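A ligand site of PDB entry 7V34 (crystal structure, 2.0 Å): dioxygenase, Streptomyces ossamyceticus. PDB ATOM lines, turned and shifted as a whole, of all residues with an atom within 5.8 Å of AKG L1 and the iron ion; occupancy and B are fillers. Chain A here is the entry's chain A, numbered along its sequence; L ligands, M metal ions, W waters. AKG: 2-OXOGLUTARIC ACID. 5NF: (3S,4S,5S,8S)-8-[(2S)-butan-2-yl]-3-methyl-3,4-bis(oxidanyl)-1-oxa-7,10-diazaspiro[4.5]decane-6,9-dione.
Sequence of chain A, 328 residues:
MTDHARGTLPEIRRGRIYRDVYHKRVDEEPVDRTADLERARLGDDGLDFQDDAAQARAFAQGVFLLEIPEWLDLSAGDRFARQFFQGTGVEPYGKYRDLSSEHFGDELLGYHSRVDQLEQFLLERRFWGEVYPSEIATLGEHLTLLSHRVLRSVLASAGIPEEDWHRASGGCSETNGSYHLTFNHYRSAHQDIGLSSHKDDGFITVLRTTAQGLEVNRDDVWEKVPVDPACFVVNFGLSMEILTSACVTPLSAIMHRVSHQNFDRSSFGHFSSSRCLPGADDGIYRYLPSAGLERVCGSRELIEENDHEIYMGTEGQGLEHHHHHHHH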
ATOM      1  N   LEU A 118       5.862 -16.077   0.274  1.00  0.00           N
ATOM      2  CA  LEU A 118       4.496 -15.549   0.333  1.00  0.00           C
ATOM      3  C   LEU A 118       3.549 -16.209  -0.663  1.00  0.00           C
ATOM      4  O   LEU A 118       3.867 -16.392  -1.837  1.00  0.00           O
ATOM      5  CB  LEU A 118       4.558 -14.056   0.047  1.00  0.00           C
ATOM      6  CG  LEU A 118       3.267 -13.248  -0.008  1.00  0.00           C
ATOM      7  CD1 LEU A 118       2.644 -13.243   1.377  1.00  0.00           C
ATOM      8  CD2 LEU A 118       3.616 -11.851  -0.444  1.00  0.00           C
ATOM      9  N   GLN A 120      -0.746 -15.255  -1.486  1.00  0.00           N
ATOM     10  CA  GLN A 120      -1.681 -14.168  -1.172  1.00  0.00           C
ATOM     11  C   GLN A 120      -3.088 -14.458  -1.671  1.00  0.00           C
ATOM     12  O   GLN A 120      -3.286 -15.207  -2.631  1.00  0.00           O
ATOM     13  CB  GLN A 120      -1.240 -12.838  -1.820  1.00  0.00           C
ATOM     14  CG  GLN A 120       0.021 -12.300  -1.255  1.00  0.00           C
ATOM     15  CD  GLN A 120       0.349 -10.950  -1.831  1.00  0.00           C
ATOM     16  OE1 GLN A 120       0.615 -10.837  -3.026  1.00  0.00           O
ATOM     17  NE2 GLN A 120       0.308  -9.908  -0.993  1.00  0.00           N
ATOM     18  N   THR A 182      -5.992  -7.582   1.312  1.00  0.00           N
ATOM     19  CA  THR A 182      -5.088  -8.605   0.814  1.00  0.00           C
ATOM     20  C   THR A 182      -4.544  -9.401   1.990  1.00  0.00           C
ATOM     21  O   THR A 182      -4.051  -8.811   2.957  1.00  0.00           O
ATOM     22  CB  THR A 182      -3.936  -7.972   0.034  1.00  0.00           C
ATOM     23  OG1 THR A 182      -4.462  -7.398  -1.167  1.00  0.00           O
ATOM     24  CG2 THR A 182      -2.832  -8.996  -0.313  1.00  0.00           C
ATOM     25  N   ASN A 184      -2.049 -12.485   3.507  1.00  0.00           N
ATOM     26  CA  ASN A 184      -0.701 -12.989   3.261  1.00  0.00           C
ATOM     27  C   ASN A 184      -0.413 -14.191   4.154  1.00  0.00           C
ATOM     28  O   ASN A 184      -0.695 -14.153   5.350  1.00  0.00           O
ATOM     29  CB  ASN A 184       0.356 -11.920   3.576  1.00  0.00           C
ATOM     30  CG  ASN A 184       0.239 -10.701   2.699  1.00  0.00           C
ATOM     31  OD1 ASN A 184      -0.184 -10.773   1.553  1.00  0.00           O
ATOM     32  ND2 ASN A 184       0.632  -9.570   3.237  1.00  0.00           N
ATOM     33  N   TYR A 186       3.025 -16.830   4.783  1.00  0.00           N
ATOM     34  CA  TYR A 186       4.407 -17.165   4.457  1.00  0.00           C
ATOM     35  C   TYR A 186       4.636 -18.659   4.652  1.00  0.00           C
ATOM     36  O   TYR A 186       4.454 -19.179   5.752  1.00  0.00           O
ATOM     37  CB  TYR A 186       5.353 -16.292   5.297  1.00  0.00           C
ATOM     38  CG  TYR A 186       5.108 -14.828   4.958  1.00  0.00           C
ATOM     39  CD1 TYR A 186       5.823 -14.215   3.932  1.00  0.00           C
ATOM     40  CD2 TYR A 186       4.081 -14.094   5.583  1.00  0.00           C
ATOM     41  CE1 TYR A 186       5.583 -12.874   3.563  1.00  0.00           C
ATOM     42  CE2 TYR A 186       3.820 -12.753   5.216  1.00  0.00           C
ATOM     43  CZ  TYR A 186       4.580 -12.148   4.210  1.00  0.00           C
ATOM     44  OH  TYR A 186       4.330 -10.840   3.819  1.00  0.00           O
ATOM     45  N   LEU A 195       9.311 -12.133   1.761  1.00  0.00           N
ATOM     46  CA  LEU A 195       8.795 -11.287   0.692  1.00  0.00           C
ATOM     47  C   LEU A 195       9.921 -10.335   0.320  1.00  0.00           C
ATOM     48  O   LEU A 195      10.482  -9.683   1.201  1.00  0.00           O
ATOM     49  CB  LEU A 195       7.526 -10.518   1.119  1.00  0.00           C
ATOM     50  CG  LEU A 195       7.055  -9.346   0.254  1.00  0.00           C
ATOM     51  CD1 LEU A 195       6.784  -9.774  -1.194  1.00  0.00           C
ATOM     52  CD2 LEU A 195       5.798  -8.699   0.855  1.00  0.00           C
ATOM     53  N   HIS A 198      10.758  -4.260  -1.368  1.00  0.00           N
ATOM     54  CA  HIS A 198       9.861  -3.599  -2.303  1.00  0.00           C
ATOM     55  C   HIS A 198       9.280  -2.344  -1.662  1.00  0.00           C
ATOM     56  O   HIS A 198       9.337  -2.139  -0.446  1.00  0.00           O
ATOM     57  CB  HIS A 198       8.719  -4.527  -2.735  1.00  0.00           C
ATOM     58  CG  HIS A 198       7.748  -4.794  -1.639  1.00  0.00           C
ATOM     59  ND1 HIS A 198       8.041  -5.616  -0.568  1.00  0.00           N
ATOM     60  CD2 HIS A 198       6.511  -4.298  -1.406  1.00  0.00           C
ATOM     61  CE1 HIS A 198       7.024  -5.635   0.264  1.00  0.00           C
ATOM     62  NE2 HIS A 198       6.078  -4.843  -0.221  1.00  0.00           N
ATOM     63  N   LYS A 199       8.685  -1.524  -2.508  1.00  0.00           N
ATOM     64  CA  LYS A 199       7.785  -0.450  -2.123  1.00  0.00           C
ATOM     65  C   LYS A 199       6.389  -0.835  -2.564  1.00  0.00           C
ATOM     66  O   LYS A 199       6.210  -1.456  -3.620  1.00  0.00           O
ATOM     67  CB  LYS A 199       8.212   0.868  -2.787  1.00  0.00           C
ATOM     68  CG  LYS A 199       9.601   1.369  -2.323  1.00  0.00           C
ATOM     69  CD  LYS A 199      10.118   2.494  -3.226  1.00  0.00           C
ATOM     70  CE  LYS A 199      11.259   3.273  -2.590  1.00  0.00           C
ATOM     71  NZ  LYS A 199      11.555   4.517  -3.357  1.00  0.00           N
ATOM     72  N   ASP A 200       5.385  -0.502  -1.745  1.00  0.00           N
ATOM     73  CA  ASP A 200       4.001  -0.713  -2.154  1.00  0.00           C
ATOM     74  C   ASP A 200       3.631   0.234  -3.281  1.00  0.00           C
ATOM     75  O   ASP A 200       4.287   1.260  -3.499  1.00  0.00           O
ATOM     76  CB  ASP A 200       3.053  -0.531  -0.970  1.00  0.00           C
ATOM     77  CG  ASP A 200       3.239  -1.601   0.081  1.00  0.00           C
ATOM     78  OD1 ASP A 200       3.868  -2.612  -0.280  1.00  0.00           O
ATOM     79  OD2 ASP A 200       2.781  -1.468   1.231  1.00  0.00           O
ATOM     80  N   THR A 205      -0.810   2.080   2.881  1.00  0.00           N
ATOM     81  CA  THR A 205      -1.044   0.699   3.277  1.00  0.00           C
ATOM     82  C   THR A 205      -1.295   0.677   4.771  1.00  0.00           C
ATOM     83  O   THR A 205      -0.503   1.221   5.549  1.00  0.00           O
ATOM     84  CB  THR A 205       0.170  -0.187   2.951  1.00  0.00           C
ATOM     85  OG1 THR A 205       0.439  -0.133   1.554  1.00  0.00           O
ATOM     86  CG2 THR A 205      -0.087  -1.643   3.371  1.00  0.00           C
ATOM     87  N   LEU A 207      -1.281  -2.022   7.496  1.00  0.00           N
ATOM     88  CA  LEU A 207      -0.825  -3.396   7.623  1.00  0.00           C
ATOM     89  C   LEU A 207      -1.132  -3.923   9.015  1.00  0.00           C
ATOM     90  O   LEU A 207      -0.749  -3.302  10.014  1.00  0.00           O
ATOM     91  CB  LEU A 207       0.673  -3.495   7.328  1.00  0.00           C
ATOM     92  CG  LEU A 207       1.232  -4.915   7.396  1.00  0.00           C
ATOM     93  CD1 LEU A 207       0.691  -5.759   6.220  1.00  0.00           C
ATOM     94  CD2 LEU A 207       2.760  -4.874   7.390  1.00  0.00           C
ATOM     95  N   THR A 209      -0.102  -6.810  11.307  1.00  0.00           N
ATOM     96  CA  THR A 209       0.886  -7.854  11.532  1.00  0.00           C
ATOM     97  C   THR A 209       1.004  -8.130  13.026  1.00  0.00           C
ATOM     98  O   THR A 209       0.970  -7.205  13.841  1.00  0.00           O
ATOM     99  CB  THR A 209       2.260  -7.447  10.937  1.00  0.00           C
ATOM    100  OG1 THR A 209       3.157  -8.547  11.065  1.00  0.00           O
ATOM    101  CG2 THR A 209       2.846  -6.231  11.651  1.00  0.00           C
ATOM    102  N   LEU A 214       8.731  -8.501   9.457  1.00  0.00           N
ATOM    103  CA  LEU A 214       8.772  -7.266   8.699  1.00  0.00           C
ATOM    104  C   LEU A 214      10.029  -6.461   9.036  1.00  0.00           C
ATOM    105  O   LEU A 214      10.339  -6.225  10.204  1.00  0.00           O
ATOM    106  CB  LEU A 214       7.515  -6.437   8.986  1.00  0.00           C
ATOM    107  CG  LEU A 214       7.349  -5.139   8.190  1.00  0.00           C
ATOM    108  CD1 LEU A 214       7.231  -5.396   6.651  1.00  0.00           C
ATOM    109  CD2 LEU A 214       6.129  -4.389   8.721  1.00  0.00           C
ATOM    110  N   ASN A 235       2.276   2.555   6.120  1.00  0.00           N
ATOM    111  CA  ASN A 235       3.336   3.123   5.313  1.00  0.00           C
ATOM    112  C   ASN A 235       2.771   3.679   4.030  1.00  0.00           C
ATOM    113  O   ASN A 235       1.609   3.440   3.667  1.00  0.00           O
ATOM    114  CB  ASN A 235       4.453   2.122   5.042  1.00  0.00           C
ATOM    115  CG  ASN A 235       3.968   0.854   4.392  1.00  0.00           C
ATOM    116  OD1 ASN A 235       3.634   0.849   3.213  1.00  0.00           O
ATOM    117  ND2 ASN A 235       3.983  -0.237   5.154  1.00  0.00           N
ATOM    118  N   HIS A 256      10.666  -2.067   2.129  1.00  0.00           N
ATOM    119  CA  HIS A 256      10.500  -3.042   3.202  1.00  0.00           C
ATOM    120  C   HIS A 256      10.456  -4.469   2.637  1.00  0.00           C
ATOM    121  O   HIS A 256      10.324  -4.699   1.437  1.00  0.00           O
ATOM    122  CB  HIS A 256       9.259  -2.733   4.032  1.00  0.00           C
ATOM    123  CG  HIS A 256       7.995  -2.662   3.239  1.00  0.00           C
ATOM    124  ND1 HIS A 256       7.715  -1.621   2.373  1.00  0.00           N
ATOM    125  CD2 HIS A 256       6.946  -3.506   3.152  1.00  0.00           C
ATOM    126  CE1 HIS A 256       6.551  -1.830   1.787  1.00  0.00           C
ATOM    127  NE2 HIS A 256       6.063  -2.976   2.254  1.00  0.00           N
ATOM    128  N   VAL A 258      10.060  -8.954   4.073  1.00  0.00           N
ATOM    129  CA  VAL A 258       9.809  -9.926   5.133  1.00  0.00           C
ATOM    130  C   VAL A 258      10.922 -10.958   5.072  1.00  0.00           C
ATOM    131  O   VAL A 258      11.134 -11.596   4.041  1.00  0.00           O
ATOM    132  CB  VAL A 258       8.433 -10.605   4.992  1.00  0.00           C
ATOM    133  CG1 VAL A 258       8.259 -11.651   6.097  1.00  0.00           C
ATOM    134  CG2 VAL A 258       7.280  -9.557   5.052  1.00  0.00           C
ATOM    135  N   ARG A 265       3.961 -17.730   8.999  1.00  0.00           N
ATOM    136  CA  ARG A 265       3.601 -16.373   9.385  1.00  0.00           C
ATOM    137  C   ARG A 265       2.419 -15.947   8.529  1.00  0.00           C
ATOM    138  O   ARG A 265       2.291 -16.370   7.375  1.00  0.00           O
ATOM    139  CB  ARG A 265       4.800 -15.427   9.206  1.00  0.00           C
ATOM    140  CG  ARG A 265       4.589 -13.967   9.677  1.00  0.00           C
ATOM    141  CD  ARG A 265       5.840 -13.124   9.327  1.00  0.00           C
ATOM    142  NE  ARG A 265       5.732 -11.717   9.702  1.00  0.00           N
ATOM    143  CZ  ARG A 265       5.164 -10.786   8.927  1.00  0.00           C
ATOM    144  NH1 ARG A 265       4.647 -11.117   7.756  1.00  0.00           N
ATOM    145  NH2 ARG A 265       5.118  -9.523   9.335  1.00  0.00           N
ATOM    146  N   SER A 266       1.533 -15.136   9.092  1.00  0.00           N
ATOM    147  CA  SER A 266       0.468 -14.541   8.297  1.00  0.00           C
ATOM    148  C   SER A 266       0.281 -13.086   8.713  1.00  0.00           C
ATOM    149  O   SER A 266       0.758 -12.652   9.761  1.00  0.00           O
ATOM    150  CB  SER A 266      -0.857 -15.332   8.405  1.00  0.00           C
ATOM    151  OG  SER A 266      -1.384 -15.257   9.723  1.00  0.00           O
ATOM    152  N   SER A 267      -0.436 -12.348   7.861  1.00  0.00           N
ATOM    153  CA  SER A 267      -0.693 -10.922   8.033  1.00  0.00           C
ATOM    154  C   SER A 267      -1.728 -10.531   6.986  1.00  0.00           C
ATOM    155  O   SER A 267      -2.055 -11.308   6.078  1.00  0.00           O
ATOM    156  CB  SER A 267       0.590 -10.098   7.878  1.00  0.00           C
ATOM    157  OG  SER A 267       1.062 -10.167   6.542  1.00  0.00           O
ATOM    158  N   PHE A 271      -4.908  -1.766   1.196  1.00  0.00           N
ATOM    159  CA  PHE A 271      -4.102  -0.993   0.272  1.00  0.00           C
ATOM    160  C   PHE A 271      -5.003  -0.006  -0.469  1.00  0.00           C
ATOM    161  O   PHE A 271      -6.046  -0.409  -1.002  1.00  0.00           O
ATOM    162  CB  PHE A 271      -3.400  -1.899  -0.752  1.00  0.00           C
ATOM    163  CG  PHE A 271      -2.375  -2.841  -0.139  1.00  0.00           C
ATOM    164  CD1 PHE A 271      -2.777  -3.988   0.531  1.00  0.00           C
ATOM    165  CD2 PHE A 271      -1.008  -2.579  -0.269  1.00  0.00           C
ATOM    166  CE1 PHE A 271      -1.820  -4.869   1.081  1.00  0.00           C
ATOM    167  CE2 PHE A 271      -0.052  -3.451   0.258  1.00  0.00           C
ATOM    168  CZ  PHE A 271      -0.462  -4.587   0.945  1.00  0.00           C
HETATM  169  C1  AKG L   1       2.816  -6.462   1.424  1.00  0.00           C
HETATM  170  O1  AKG L   1       3.043  -5.615   0.529  1.00  0.00           O
HETATM  171  O2  AKG L   1       1.844  -7.221   1.315  1.00  0.00           O
HETATM  172  C2  AKG L   1       3.686  -6.583   2.588  1.00  0.00           C
HETATM  173  O5  AKG L   1       4.659  -5.861   2.723  1.00  0.00           O
HETATM  174  C3  AKG L   1       3.381  -7.610   3.666  1.00  0.00           C
HETATM  175  C4  AKG L   1       4.280  -7.292   4.872  1.00  0.00           C
HETATM  176  C5  AKG L   1       4.018  -8.284   5.999  1.00  0.00           C
HETATM  177  O3  AKG L   1       4.306  -7.959   7.160  1.00  0.00           O
HETATM  178  O4  AKG L   1       3.486  -9.395   5.741  1.00  0.00           O
HETATM  179  C1  5NF L   2       1.982  -6.650  -4.495  1.00  0.00           C
HETATM  180  C2  5NF L   2       2.583  -6.916  -3.114  1.00  0.00           C
HETATM  181  C3  5NF L   2       1.565  -6.155  -2.121  1.00  0.00           C
HETATM  182  C4  5NF L   2       0.443  -5.573  -3.060  1.00  0.00           C
HETATM  183  C5  5NF L   2       0.511  -4.061  -3.427  1.00  0.00           C
HETATM  184  C6  5NF L   2      -2.032  -5.177  -2.777  1.00  0.00           C
HETATM  185  C10 5NF L   2      -2.109  -5.064  -5.788  1.00  0.00           C
HETATM  186  C11 5NF L   2      -2.973  -5.430  -7.003  1.00  0.00           C
HETATM  187  C12 5NF L   2       4.043  -6.438  -3.040  1.00  0.00           C
HETATM  188  C7  5NF L   2      -2.022  -3.825  -3.541  1.00  0.00           C
HETATM  189  C8  5NF L   2      -2.739  -3.982  -4.915  1.00  0.00           C
HETATM  190  C9  5NF L   2      -2.728  -2.622  -5.672  1.00  0.00           C
HETATM  191  N1  5NF L   2      -0.878  -5.907  -2.607  1.00  0.00           N
HETATM  192  N2  5NF L   2      -0.645  -3.331  -3.627  1.00  0.00           N
HETATM  193  O1  5NF L   2       2.522  -8.260  -2.841  1.00  0.00           O
HETATM  194  O2  5NF L   2       0.940  -7.032  -1.228  1.00  0.00           O
HETATM  195  O3  5NF L   2       0.662  -6.216  -4.322  1.00  0.00           O
HETATM  196  O4  5NF L   2       1.605  -3.493  -3.531  1.00  0.00           O
HETATM  197  O5  5NF L   2      -3.036  -5.671  -2.288  1.00  0.00           O
HETATM  198 FE    FE M   1       4.499  -4.135   1.201  1.00  0.00          FE
HETATM  199  O   HOH W   1       2.962  -3.527   2.889  1.00  0.00           O
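O3 of AKG L1 is in salt-bridge range of NH2 of Arg 265 (2.8 Å).
O4 of AKG L1 sits at hydrogen-bond distance from OG of Ser 267, at 2.7 Å.
NE2 of Gln 120 is in hydrogen-bond range of O2 of 5NF L2 (3.0 Å).
OG1 of Thr 182 sits at hydrogen-bond distance from O5 of 5NF L2.
ND2 of Asn 184 is in hydrogen-bond range of O2 of AKG L1 (3.3 Å).
The side-chain hydroxyl (OH) of Tyr 186 lies within hydrogen-bond range of an oxygen (O4) of AKG L1 (2.5 Å).
O2 of 5NF L2 lies within hydrogen-bond range of O2 of AKG L1, at 2.7 Å.
O of Ser 267 sits at hydrogen-bond distance from N of Asn 184 (2.8 Å).
The backbone NH (N) of Tyr 186 is in hydrogen-bond range of the backbone carbonyl oxygen (O) of Arg 265.
The side-chain amide oxygen of Asn 184 lies within hydrogen-bond range of the side-chain amide nitrogen of Gln 120, 2.7 Å away.
The side-chain hydroxyl (OG1) of Thr 209 is in hydrogen-bond range of the guanidinium group (NH2) of Arg 265, 2.8 Å away.
The backbone NH of Leu 195 sits at hydrogen-bond distance from the backbone carbonyl oxygen of Val 258 (3.0 Å).
OD2 of Asp 200 sits close to OD1 of Asn 235 (3.2 Å).
The side-chain carboxylate (OD2) of Asp 200 lies within hydrogen-bond range of the side-chain hydroxyl (OG1) of Thr 205 (2.7 Å).
Gln 120 touches AKG L1 (NE2 to O2, 3.9 Å).
CD2 of Leu 195 touches C2 of AKG L1, 3.5 Å away.
CD2 of Leu 207 touches O3 of AKG L1, 3.5 Å away.
Leu 214 touches AKG L1 (CD1 to O3, 3.9 Å).
CG2 of Val 258 touches C5 of AKG L1 (3.6 Å).
Phe 271 touches AKG L1 (CZ to O2, 3.5 Å).
Hydrophobic or aromatic side chains within 4 Å of AKG L1: Tyr 186, Leu 195, His 198, Leu 207, Leu 214, His 256, Val 258 and Phe 271.
Of the 20 residues printed, 13 come within 4 Å of AKG L1.
The nearest printed residue that does not touch the iron ion is Phe 271 (4.7 Å).
The iron ion is bound by an oxygen (O1) of AKG L1 (2.2 Å), a ring nitrogen (NE2) of His 256 (2.2 Å), the side-chain carboxylate of Asp 200 (2.2 Å), a ring nitrogen (NE2) of His 198 (2.2 Å), an oxygen (O5) of AKG L1 (2.3 Å) and water W1 (2.4 Å).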
